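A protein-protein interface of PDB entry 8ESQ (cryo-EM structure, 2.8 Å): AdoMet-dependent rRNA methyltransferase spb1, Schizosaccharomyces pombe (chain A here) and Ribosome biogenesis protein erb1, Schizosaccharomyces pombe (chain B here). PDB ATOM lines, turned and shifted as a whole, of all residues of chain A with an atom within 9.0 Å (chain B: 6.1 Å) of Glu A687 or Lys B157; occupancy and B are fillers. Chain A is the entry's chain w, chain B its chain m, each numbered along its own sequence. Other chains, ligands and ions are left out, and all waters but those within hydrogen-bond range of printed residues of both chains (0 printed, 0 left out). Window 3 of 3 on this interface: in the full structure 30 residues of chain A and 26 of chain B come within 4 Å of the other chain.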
ATOM      1  N   VAL A 619      -7.952   4.667   7.415  1.00  0.00           N
ATOM      2  CA  VAL A 619      -8.193   4.159   8.760  1.00  0.00           C
ATOM      3  C   VAL A 619      -7.261   4.905   9.701  1.00  0.00           C
ATOM      4  O   VAL A 619      -6.146   5.278   9.327  1.00  0.00           O
ATOM      5  CB  VAL A 619      -7.996   2.623   8.833  1.00  0.00           C
ATOM      6  CG1 VAL A 619      -6.537   2.254   8.658  1.00  0.00           C
ATOM      7  CG2 VAL A 619      -8.535   2.073  10.144  1.00  0.00           C
ATOM      8  N   MET A 627      -3.461  -1.166  17.704  1.00  0.00           N
ATOM      9  CA  MET A 627      -2.009  -1.027  17.658  1.00  0.00           C
ATOM     10  C   MET A 627      -1.304  -2.354  17.909  1.00  0.00           C
ATOM     11  O   MET A 627      -0.344  -2.686  17.207  1.00  0.00           O
ATOM     12  CB  MET A 627      -1.549   0.023  18.663  1.00  0.00           C
ATOM     13  CG  MET A 627      -0.403   0.886  18.165  1.00  0.00           C
ATOM     14  SD  MET A 627      -0.535   1.337  16.430  1.00  0.00           S
ATOM     15  CE  MET A 627       0.989   2.246  16.224  1.00  0.00           C
ATOM     16  N   GLN A 631       1.046  -3.769  15.308  1.00  0.00           N
ATOM     17  CA  GLN A 631       2.432  -4.059  15.656  1.00  0.00           C
ATOM     18  C   GLN A 631       2.789  -5.503  15.332  1.00  0.00           C
ATOM     19  O   GLN A 631       3.885  -5.780  14.837  1.00  0.00           O
ATOM     20  CB  GLN A 631       2.678  -3.759  17.133  1.00  0.00           C
ATOM     21  CG  GLN A 631       2.844  -2.282  17.436  1.00  0.00           C
ATOM     22  CD  GLN A 631       3.285  -2.025  18.861  1.00  0.00           C
ATOM     23  OE1 GLN A 631       3.369  -2.945  19.672  1.00  0.00           O
ATOM     24  NE2 GLN A 631       3.574  -0.768  19.173  1.00  0.00           N
ATOM     25  N   GLU A 680       3.988  -1.879  24.586  1.00  0.00           N
ATOM     26  CA  GLU A 680       4.621  -1.235  23.441  1.00  0.00           C
ATOM     27  C   GLU A 680       3.602  -0.464  22.613  1.00  0.00           C
ATOM     28  O   GLU A 680       3.886   0.641  22.134  1.00  0.00           O
ATOM     29  CB  GLU A 680       5.329  -2.282  22.582  1.00  0.00           C
ATOM     30  CG  GLU A 680       6.581  -2.854  23.220  1.00  0.00           C
ATOM     31  CD  GLU A 680       6.322  -4.165  23.934  1.00  0.00           C
ATOM     32  OE1 GLU A 680       5.189  -4.365  24.420  1.00  0.00           O
ATOM     33  OE2 GLU A 680       7.251  -4.997  24.009  1.00  0.00           O
ATOM     34  N   ALA A 681       2.410  -1.032  22.431  1.00  0.00           N
ATOM     35  CA  ALA A 681       1.366  -0.340  21.685  1.00  0.00           C
ATOM     36  C   ALA A 681       0.836   0.865  22.452  1.00  0.00           C
ATOM     37  O   ALA A 681       0.450   1.872  21.848  1.00  0.00           O
ATOM     38  CB  ALA A 681       0.236  -1.308  21.356  1.00  0.00           C
ATOM     39  N   VAL A 682       0.791   0.774  23.783  1.00  0.00           N
ATOM     40  CA  VAL A 682       0.334   1.903  24.589  1.00  0.00           C
ATOM     41  C   VAL A 682       1.274   3.090  24.420  1.00  0.00           C
ATOM     42  O   VAL A 682       0.832   4.238  24.290  1.00  0.00           O
ATOM     43  CB  VAL A 682       0.203   1.488  26.065  1.00  0.00           C
ATOM     44  CG1 VAL A 682      -0.248   2.666  26.910  1.00  0.00           C
ATOM     45  CG2 VAL A 682      -0.766   0.330  26.205  1.00  0.00           C
ATOM     46  N   LEU A 683       2.584   2.832  24.422  1.00  0.00           N
ATOM     47  CA  LEU A 683       3.550   3.898  24.175  1.00  0.00           C
ATOM     48  C   LEU A 683       3.375   4.485  22.781  1.00  0.00           C
ATOM     49  O   LEU A 683       3.516   5.698  22.588  1.00  0.00           O
ATOM     50  CB  LEU A 683       4.974   3.374  24.358  1.00  0.00           C
ATOM     51  CG  LEU A 683       5.276   2.603  25.644  1.00  0.00           C
ATOM     52  CD1 LEU A 683       6.653   1.963  25.574  1.00  0.00           C
ATOM     53  CD2 LEU A 683       5.170   3.518  26.849  1.00  0.00           C
ATOM     54  N   ALA A 684       3.075   3.637  21.794  1.00  0.00           N
ATOM     55  CA  ALA A 684       2.894   4.121  20.430  1.00  0.00           C
ATOM     56  C   ALA A 684       1.720   5.085  20.334  1.00  0.00           C
ATOM     57  O   ALA A 684       1.796   6.097  19.627  1.00  0.00           O
ATOM     58  CB  ALA A 684       2.701   2.942  19.477  1.00  0.00           C
ATOM     59  N   LEU A 685       0.619   4.787  21.029  1.00  0.00           N
ATOM     60  CA  LEU A 685      -0.516   5.704  21.034  1.00  0.00           C
ATOM     61  C   LEU A 685      -0.161   7.024  21.700  1.00  0.00           C
ATOM     62  O   LEU A 685      -0.504   8.096  21.188  1.00  0.00           O
ATOM     63  CB  LEU A 685      -1.720   5.070  21.727  1.00  0.00           C
ATOM     64  CG  LEU A 685      -2.735   4.403  20.805  1.00  0.00           C
ATOM     65  CD1 LEU A 685      -3.372   5.456  19.924  1.00  0.00           C
ATOM     66  CD2 LEU A 685      -2.089   3.336  19.966  1.00  0.00           C
ATOM     67  N   ARG A 686       0.520   6.971  22.847  1.00  0.00           N
ATOM     68  CA  ARG A 686       0.949   8.205  23.497  1.00  0.00           C
ATOM     69  C   ARG A 686       1.857   9.010  22.579  1.00  0.00           C
ATOM     70  O   ARG A 686       1.813  10.246  22.576  1.00  0.00           O
ATOM     71  CB  ARG A 686       1.656   7.893  24.815  1.00  0.00           C
ATOM     72  CG  ARG A 686       0.795   7.162  25.833  1.00  0.00           C
ATOM     73  CD  ARG A 686       1.365   7.311  27.235  1.00  0.00           C
ATOM     74  NE  ARG A 686       0.750   6.388  28.182  1.00  0.00           N
ATOM     75  CZ  ARG A 686       1.342   5.300  28.658  1.00  0.00           C
ATOM     76  NH1 ARG A 686       2.569   4.967  28.297  1.00  0.00           N
ATOM     77  NH2 ARG A 686       0.686   4.530  29.521  1.00  0.00           N
ATOM     78  N   GLU A 687       2.690   8.324  21.795  1.00  0.00           N
ATOM     79  CA  GLU A 687       3.519   9.013  20.814  1.00  0.00           C
ATOM     80  C   GLU A 687       2.665   9.650  19.723  1.00  0.00           C
ATOM     81  O   GLU A 687       2.914  10.791  19.317  1.00  0.00           O
ATOM     82  CB  GLU A 687       4.532   8.039  20.214  1.00  0.00           C
ATOM     83  CG  GLU A 687       5.814   8.695  19.741  1.00  0.00           C
ATOM     84  CD  GLU A 687       5.653   9.388  18.407  1.00  0.00           C
ATOM     85  OE1 GLU A 687       4.774   8.971  17.624  1.00  0.00           O
ATOM     86  OE2 GLU A 687       6.399  10.354  18.142  1.00  0.00           O
ATOM     87  N   LYS A 688       1.658   8.924  19.228  1.00  0.00           N
ATOM     88  CA  LYS A 688       0.742   9.503  18.247  1.00  0.00           C
ATOM     89  C   LYS A 688      -0.041  10.667  18.838  1.00  0.00           C
ATOM     90  O   LYS A 688      -0.188  11.715  18.199  1.00  0.00           O
ATOM     91  CB  LYS A 688      -0.219   8.438  17.723  1.00  0.00           C
ATOM     92  CG  LYS A 688       0.409   7.365  16.856  1.00  0.00           C
ATOM     93  CD  LYS A 688      -0.624   6.810  15.885  1.00  0.00           C
ATOM     94  CE  LYS A 688       0.015   6.285  14.614  1.00  0.00           C
ATOM     95  NZ  LYS A 688      -1.003   5.825  13.630  1.00  0.00           N
ATOM     96  N   MET A 689      -0.554  10.502  20.058  1.00  0.00           N
ATOM     97  CA  MET A 689      -1.362  11.545  20.676  1.00  0.00           C
ATOM     98  C   MET A 689      -0.531  12.741  21.118  1.00  0.00           C
ATOM     99  O   MET A 689      -1.102  13.775  21.479  1.00  0.00           O
ATOM    100  CB  MET A 689      -2.138  10.977  21.864  1.00  0.00           C
ATOM    101  CG  MET A 689      -3.422  10.249  21.484  1.00  0.00           C
ATOM    102  SD  MET A 689      -3.228   9.120  20.090  1.00  0.00           S
ATOM    103  CE  MET A 689      -4.263   9.906  18.858  1.00  0.00           C
ATOM    104  N   LYS A 690       0.797  12.625  21.110  1.00  0.00           N
ATOM    105  CA  LYS A 690       1.652  13.749  21.466  1.00  0.00           C
ATOM    106  C   LYS A 690       1.573  14.836  20.404  1.00  0.00           C
ATOM    107  O   LYS A 690       2.127  14.687  19.310  1.00  0.00           O
ATOM    108  CB  LYS A 690       3.098  13.289  21.651  1.00  0.00           C
ATOM    109  CG  LYS A 690       4.060  14.416  21.986  1.00  0.00           C
ATOM    110  CD  LYS A 690       5.470  13.899  22.200  1.00  0.00           C
ATOM    111  CE  LYS A 690       5.596  13.183  23.534  1.00  0.00           C
ATOM    112  NZ  LYS A 690       5.431  14.119  24.679  1.00  0.00           N
ATOM    113  N   ALA A 691       0.884  15.929  20.717  1.00  0.00           N
ATOM    114  CA  ALA A 691       0.734  17.020  19.770  1.00  0.00           C
ATOM    115  C   ALA A 691       2.046  17.785  19.614  1.00  0.00           C
ATOM    116  O   ALA A 691       2.943  17.717  20.457  1.00  0.00           O
ATOM    117  CB  ALA A 691      -0.377  17.969  20.216  1.00  0.00           C
ATOM    118  N   LEU A 692       2.146  18.520  18.504  1.00  0.00           N
ATOM    119  CA  LEU A 692       3.351  19.298  18.236  1.00  0.00           C
ATOM    120  C   LEU A 692       3.583  20.366  19.296  1.00  0.00           C
ATOM    121  O   LEU A 692       4.732  20.735  19.563  1.00  0.00           O
ATOM    122  CB  LEU A 692       3.267  19.941  16.853  1.00  0.00           C
ATOM    123  CG  LEU A 692       3.634  19.064  15.656  1.00  0.00           C
ATOM    124  CD1 LEU A 692       2.511  18.099  15.312  1.00  0.00           C
ATOM    125  CD2 LEU A 692       3.981  19.935  14.466  1.00  0.00           C
ATOM    126  N   ALA A 694       2.436  20.002  22.499  1.00  0.00           N
ATOM    127  CA  ALA A 694       2.137  19.395  23.792  1.00  0.00           C
ATOM    128  C   ALA A 694       3.082  19.900  24.873  1.00  0.00           C
ATOM    129  O   ALA A 694       2.658  20.172  26.002  1.00  0.00           O
ATOM    130  CB  ALA A 694       2.206  17.871  23.684  1.00  0.00           C
ATOM    131  N   ILE B 152      10.226  15.410   8.942  1.00  0.00           N
ATOM    132  CA  ILE B 152       8.919  15.400   8.288  1.00  0.00           C
ATOM    133  C   ILE B 152       8.110  14.191   8.734  1.00  0.00           C
ATOM    134  O   ILE B 152       6.957  14.323   9.160  1.00  0.00           O
ATOM    135  CB  ILE B 152       9.074  15.437   6.757  1.00  0.00           C
ATOM    136  CG1 ILE B 152       9.462  16.838   6.290  1.00  0.00           C
ATOM    137  CG2 ILE B 152       7.799  14.969   6.074  1.00  0.00           C
ATOM    138  CD1 ILE B 152       9.685  16.934   4.804  1.00  0.00           C
ATOM    139  N   ALA B 153       8.711  13.000   8.672  1.00  0.00           N
ATOM    140  CA  ALA B 153       7.994  11.791   9.064  1.00  0.00           C
ATOM    141  C   ALA B 153       7.544  11.866  10.516  1.00  0.00           C
ATOM    142  O   ALA B 153       6.433  11.439  10.852  1.00  0.00           O
ATOM    143  CB  ALA B 153       8.870  10.561   8.833  1.00  0.00           C
ATOM    144  N   SER B 154       8.393  12.404  11.393  1.00  0.00           N
ATOM    145  CA  SER B 154       7.992  12.596  12.781  1.00  0.00           C
ATOM    146  C   SER B 154       6.866  13.617  12.897  1.00  0.00           C
ATOM    147  O   SER B 154       5.947  13.447  13.706  1.00  0.00           O
ATOM    148  CB  SER B 154       9.194  13.024  13.621  1.00  0.00           C
ATOM    149  OG  SER B 154       8.788  13.456  14.908  1.00  0.00           O
ATOM    150  N   ILE B 155       6.925  14.693  12.107  1.00  0.00           N
ATOM    151  CA  ILE B 155       5.888  15.719  12.179  1.00  0.00           C
ATOM    152  C   ILE B 155       4.550  15.159  11.712  1.00  0.00           C
ATOM    153  O   ILE B 155       3.533  15.279  12.404  1.00  0.00           O
ATOM    154  CB  ILE B 155       6.294  16.961  11.364  1.00  0.00           C
ATOM    155  CG1 ILE B 155       7.409  17.729  12.075  1.00  0.00           C
ATOM    156  CG2 ILE B 155       5.092  17.864  11.142  1.00  0.00           C
ATOM    157  CD1 ILE B 155       7.010  18.284  13.418  1.00  0.00           C
ATOM    158  N   ASP B 156       4.531  14.528  10.539  1.00  0.00           N
ATOM    159  CA  ASP B 156       3.320  13.906  10.003  1.00  0.00           C
ATOM    160  C   ASP B 156       3.556  12.402   9.857  1.00  0.00           C
ATOM    161  O   ASP B 156       4.148  11.916   8.893  1.00  0.00           O
ATOM    162  CB  ASP B 156       2.831  14.623   8.633  1.00  0.00           C
ATOM    163  CG  ASP B 156       3.683  14.282   7.418  1.00  0.00           C
ATOM    164  OD1 ASP B 156       4.876  13.957   7.569  1.00  0.00           O
ATOM    165  OD2 ASP B 156       3.169  14.412   6.287  1.00  0.00           O
ATOM    166  N   LYS B 157       3.101  11.657  10.863  1.00  0.00           N
ATOM    167  CA  LYS B 157       3.224  10.207  10.851  1.00  0.00           C
ATOM    168  C   LYS B 157       2.520   9.626   9.634  1.00  0.00           C
ATOM    169  O   LYS B 157       1.414  10.042   9.280  1.00  0.00           O
ATOM    170  CB  LYS B 157       2.632   9.624  12.134  1.00  0.00           C
ATOM    171  CG  LYS B 157       3.200  10.239  13.395  1.00  0.00           C
ATOM    172  CD  LYS B 157       4.687   9.975  13.516  1.00  0.00           C
ATOM    173  CE  LYS B 157       5.220  10.491  14.837  1.00  0.00           C
ATOM    174  NZ  LYS B 157       4.179  10.443  15.898  1.00  0.00           N
ATOM    175  N   ASP B 158       3.175   8.666   8.992  1.00  0.00           N
ATOM    176  CA  ASP B 158       2.590   8.013   7.833  1.00  0.00           C
ATOM    177  C   ASP B 158       1.343   7.243   8.245  1.00  0.00           C
ATOM    178  O   ASP B 158       1.212   6.791   9.385  1.00  0.00           O
ATOM    179  CB  ASP B 158       3.604   7.069   7.185  1.00  0.00           C
ATOM    180  CG  ASP B 158       3.100   6.458   5.885  1.00  0.00           C
ATOM    181  OD1 ASP B 158       1.956   6.746   5.477  1.00  0.00           O
ATOM    182  OD2 ASP B 158       3.857   5.677   5.271  1.00  0.00           O
ATOM    183  N   LYS B 159       0.409   7.115   7.305  1.00  0.00           N
ATOM    184  CA  LYS B 159      -0.781   6.319   7.557  1.00  0.00           C
ATOM    185  C   LYS B 159      -0.379   4.884   7.866  1.00  0.00           C
ATOM    186  O   LYS B 159       0.416   4.275   7.146  1.00  0.00           O
ATOM    187  CB  LYS B 159      -1.715   6.371   6.348  1.00  0.00           C
ATOM    188  CG  LYS B 159      -3.077   5.747   6.581  1.00  0.00           C
ATOM    189  CD  LYS B 159      -3.943   5.861   5.339  1.00  0.00           C
ATOM    190  CE  LYS B 159      -4.298   7.311   5.051  1.00  0.00           C
ATOM    191  NZ  LYS B 159      -5.134   7.450   3.827  1.00  0.00           N
ATOM    192  N   TRP B 161       1.307   4.139  10.708  1.00  0.00           N
ATOM    193  CA  TRP B 161       2.619   4.228  11.344  1.00  0.00           C
ATOM    194  C   TRP B 161       2.651   3.248  12.504  1.00  0.00           C
ATOM    195  O   TRP B 161       2.039   3.481  13.547  1.00  0.00           O
ATOM    196  CB  TRP B 161       2.900   5.646  11.827  1.00  0.00           C
ATOM    197  CG  TRP B 161       4.172   5.760  12.612  1.00  0.00           C
ATOM    198  CD1 TRP B 161       5.439   5.826  12.113  1.00  0.00           C
ATOM    199  CD2 TRP B 161       4.301   5.807  14.038  1.00  0.00           C
ATOM    200  NE1 TRP B 161       6.348   5.919  13.138  1.00  0.00           N
ATOM    201  CE2 TRP B 161       5.675   5.908  14.330  1.00  0.00           C
ATOM    202  CE3 TRP B 161       3.388   5.778  15.095  1.00  0.00           C
ATOM    203  CZ2 TRP B 161       6.156   5.980  15.635  1.00  0.00           C
ATOM    204  CZ3 TRP B 161       3.867   5.847  16.389  1.00  0.00           C
ATOM    205  CH2 TRP B 161       5.239   5.947  16.648  1.00  0.00           C
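Among the printed residues, pairs that only touch across the chains: Met A627 with Trp B161, Ala A684 with Trp B161, Glu A687 with Trp B161, Lys A688 with Trp B161 and Leu A692 with Ile B155.
Of the 17 printed residues of chain A, 5 touch a printed residue of chain B.
Hydrophobic or aromatic side chains of chain B within 4 Å of the printed part of chain A: Ile B155 and Trp B161.
Among the printed residues, 6 pairs touch across the chains.
Of the printed residues of chain B, Met A627 touches Trp B161 (3.1 Å).
Of the printed residues of chain B, Ala A684 touches Trp B161 (3.9 Å).
Arg A686 touches none of the printed residues of chain B.
Of the printed residues of chain B, Lys A688 touches Trp B161.
Ala A694 touches none of the printed residues of chain B.
No residue of chain A comes within 4 Å of Ser B154.
Lys B157 touches just one residue of chain A: Glu A687.
The nearest residue of chain B that does not touch Glu A687 is Ser B154 (5.1 Å).
The nearest residue of chain A that does not touch Lys B157 is Lys A688 (4.3 Å).
The side-chain carboxylate (OE2) of Glu A687 lies within salt-bridge range of the side-chain amino group (NZ) of Lys B157.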
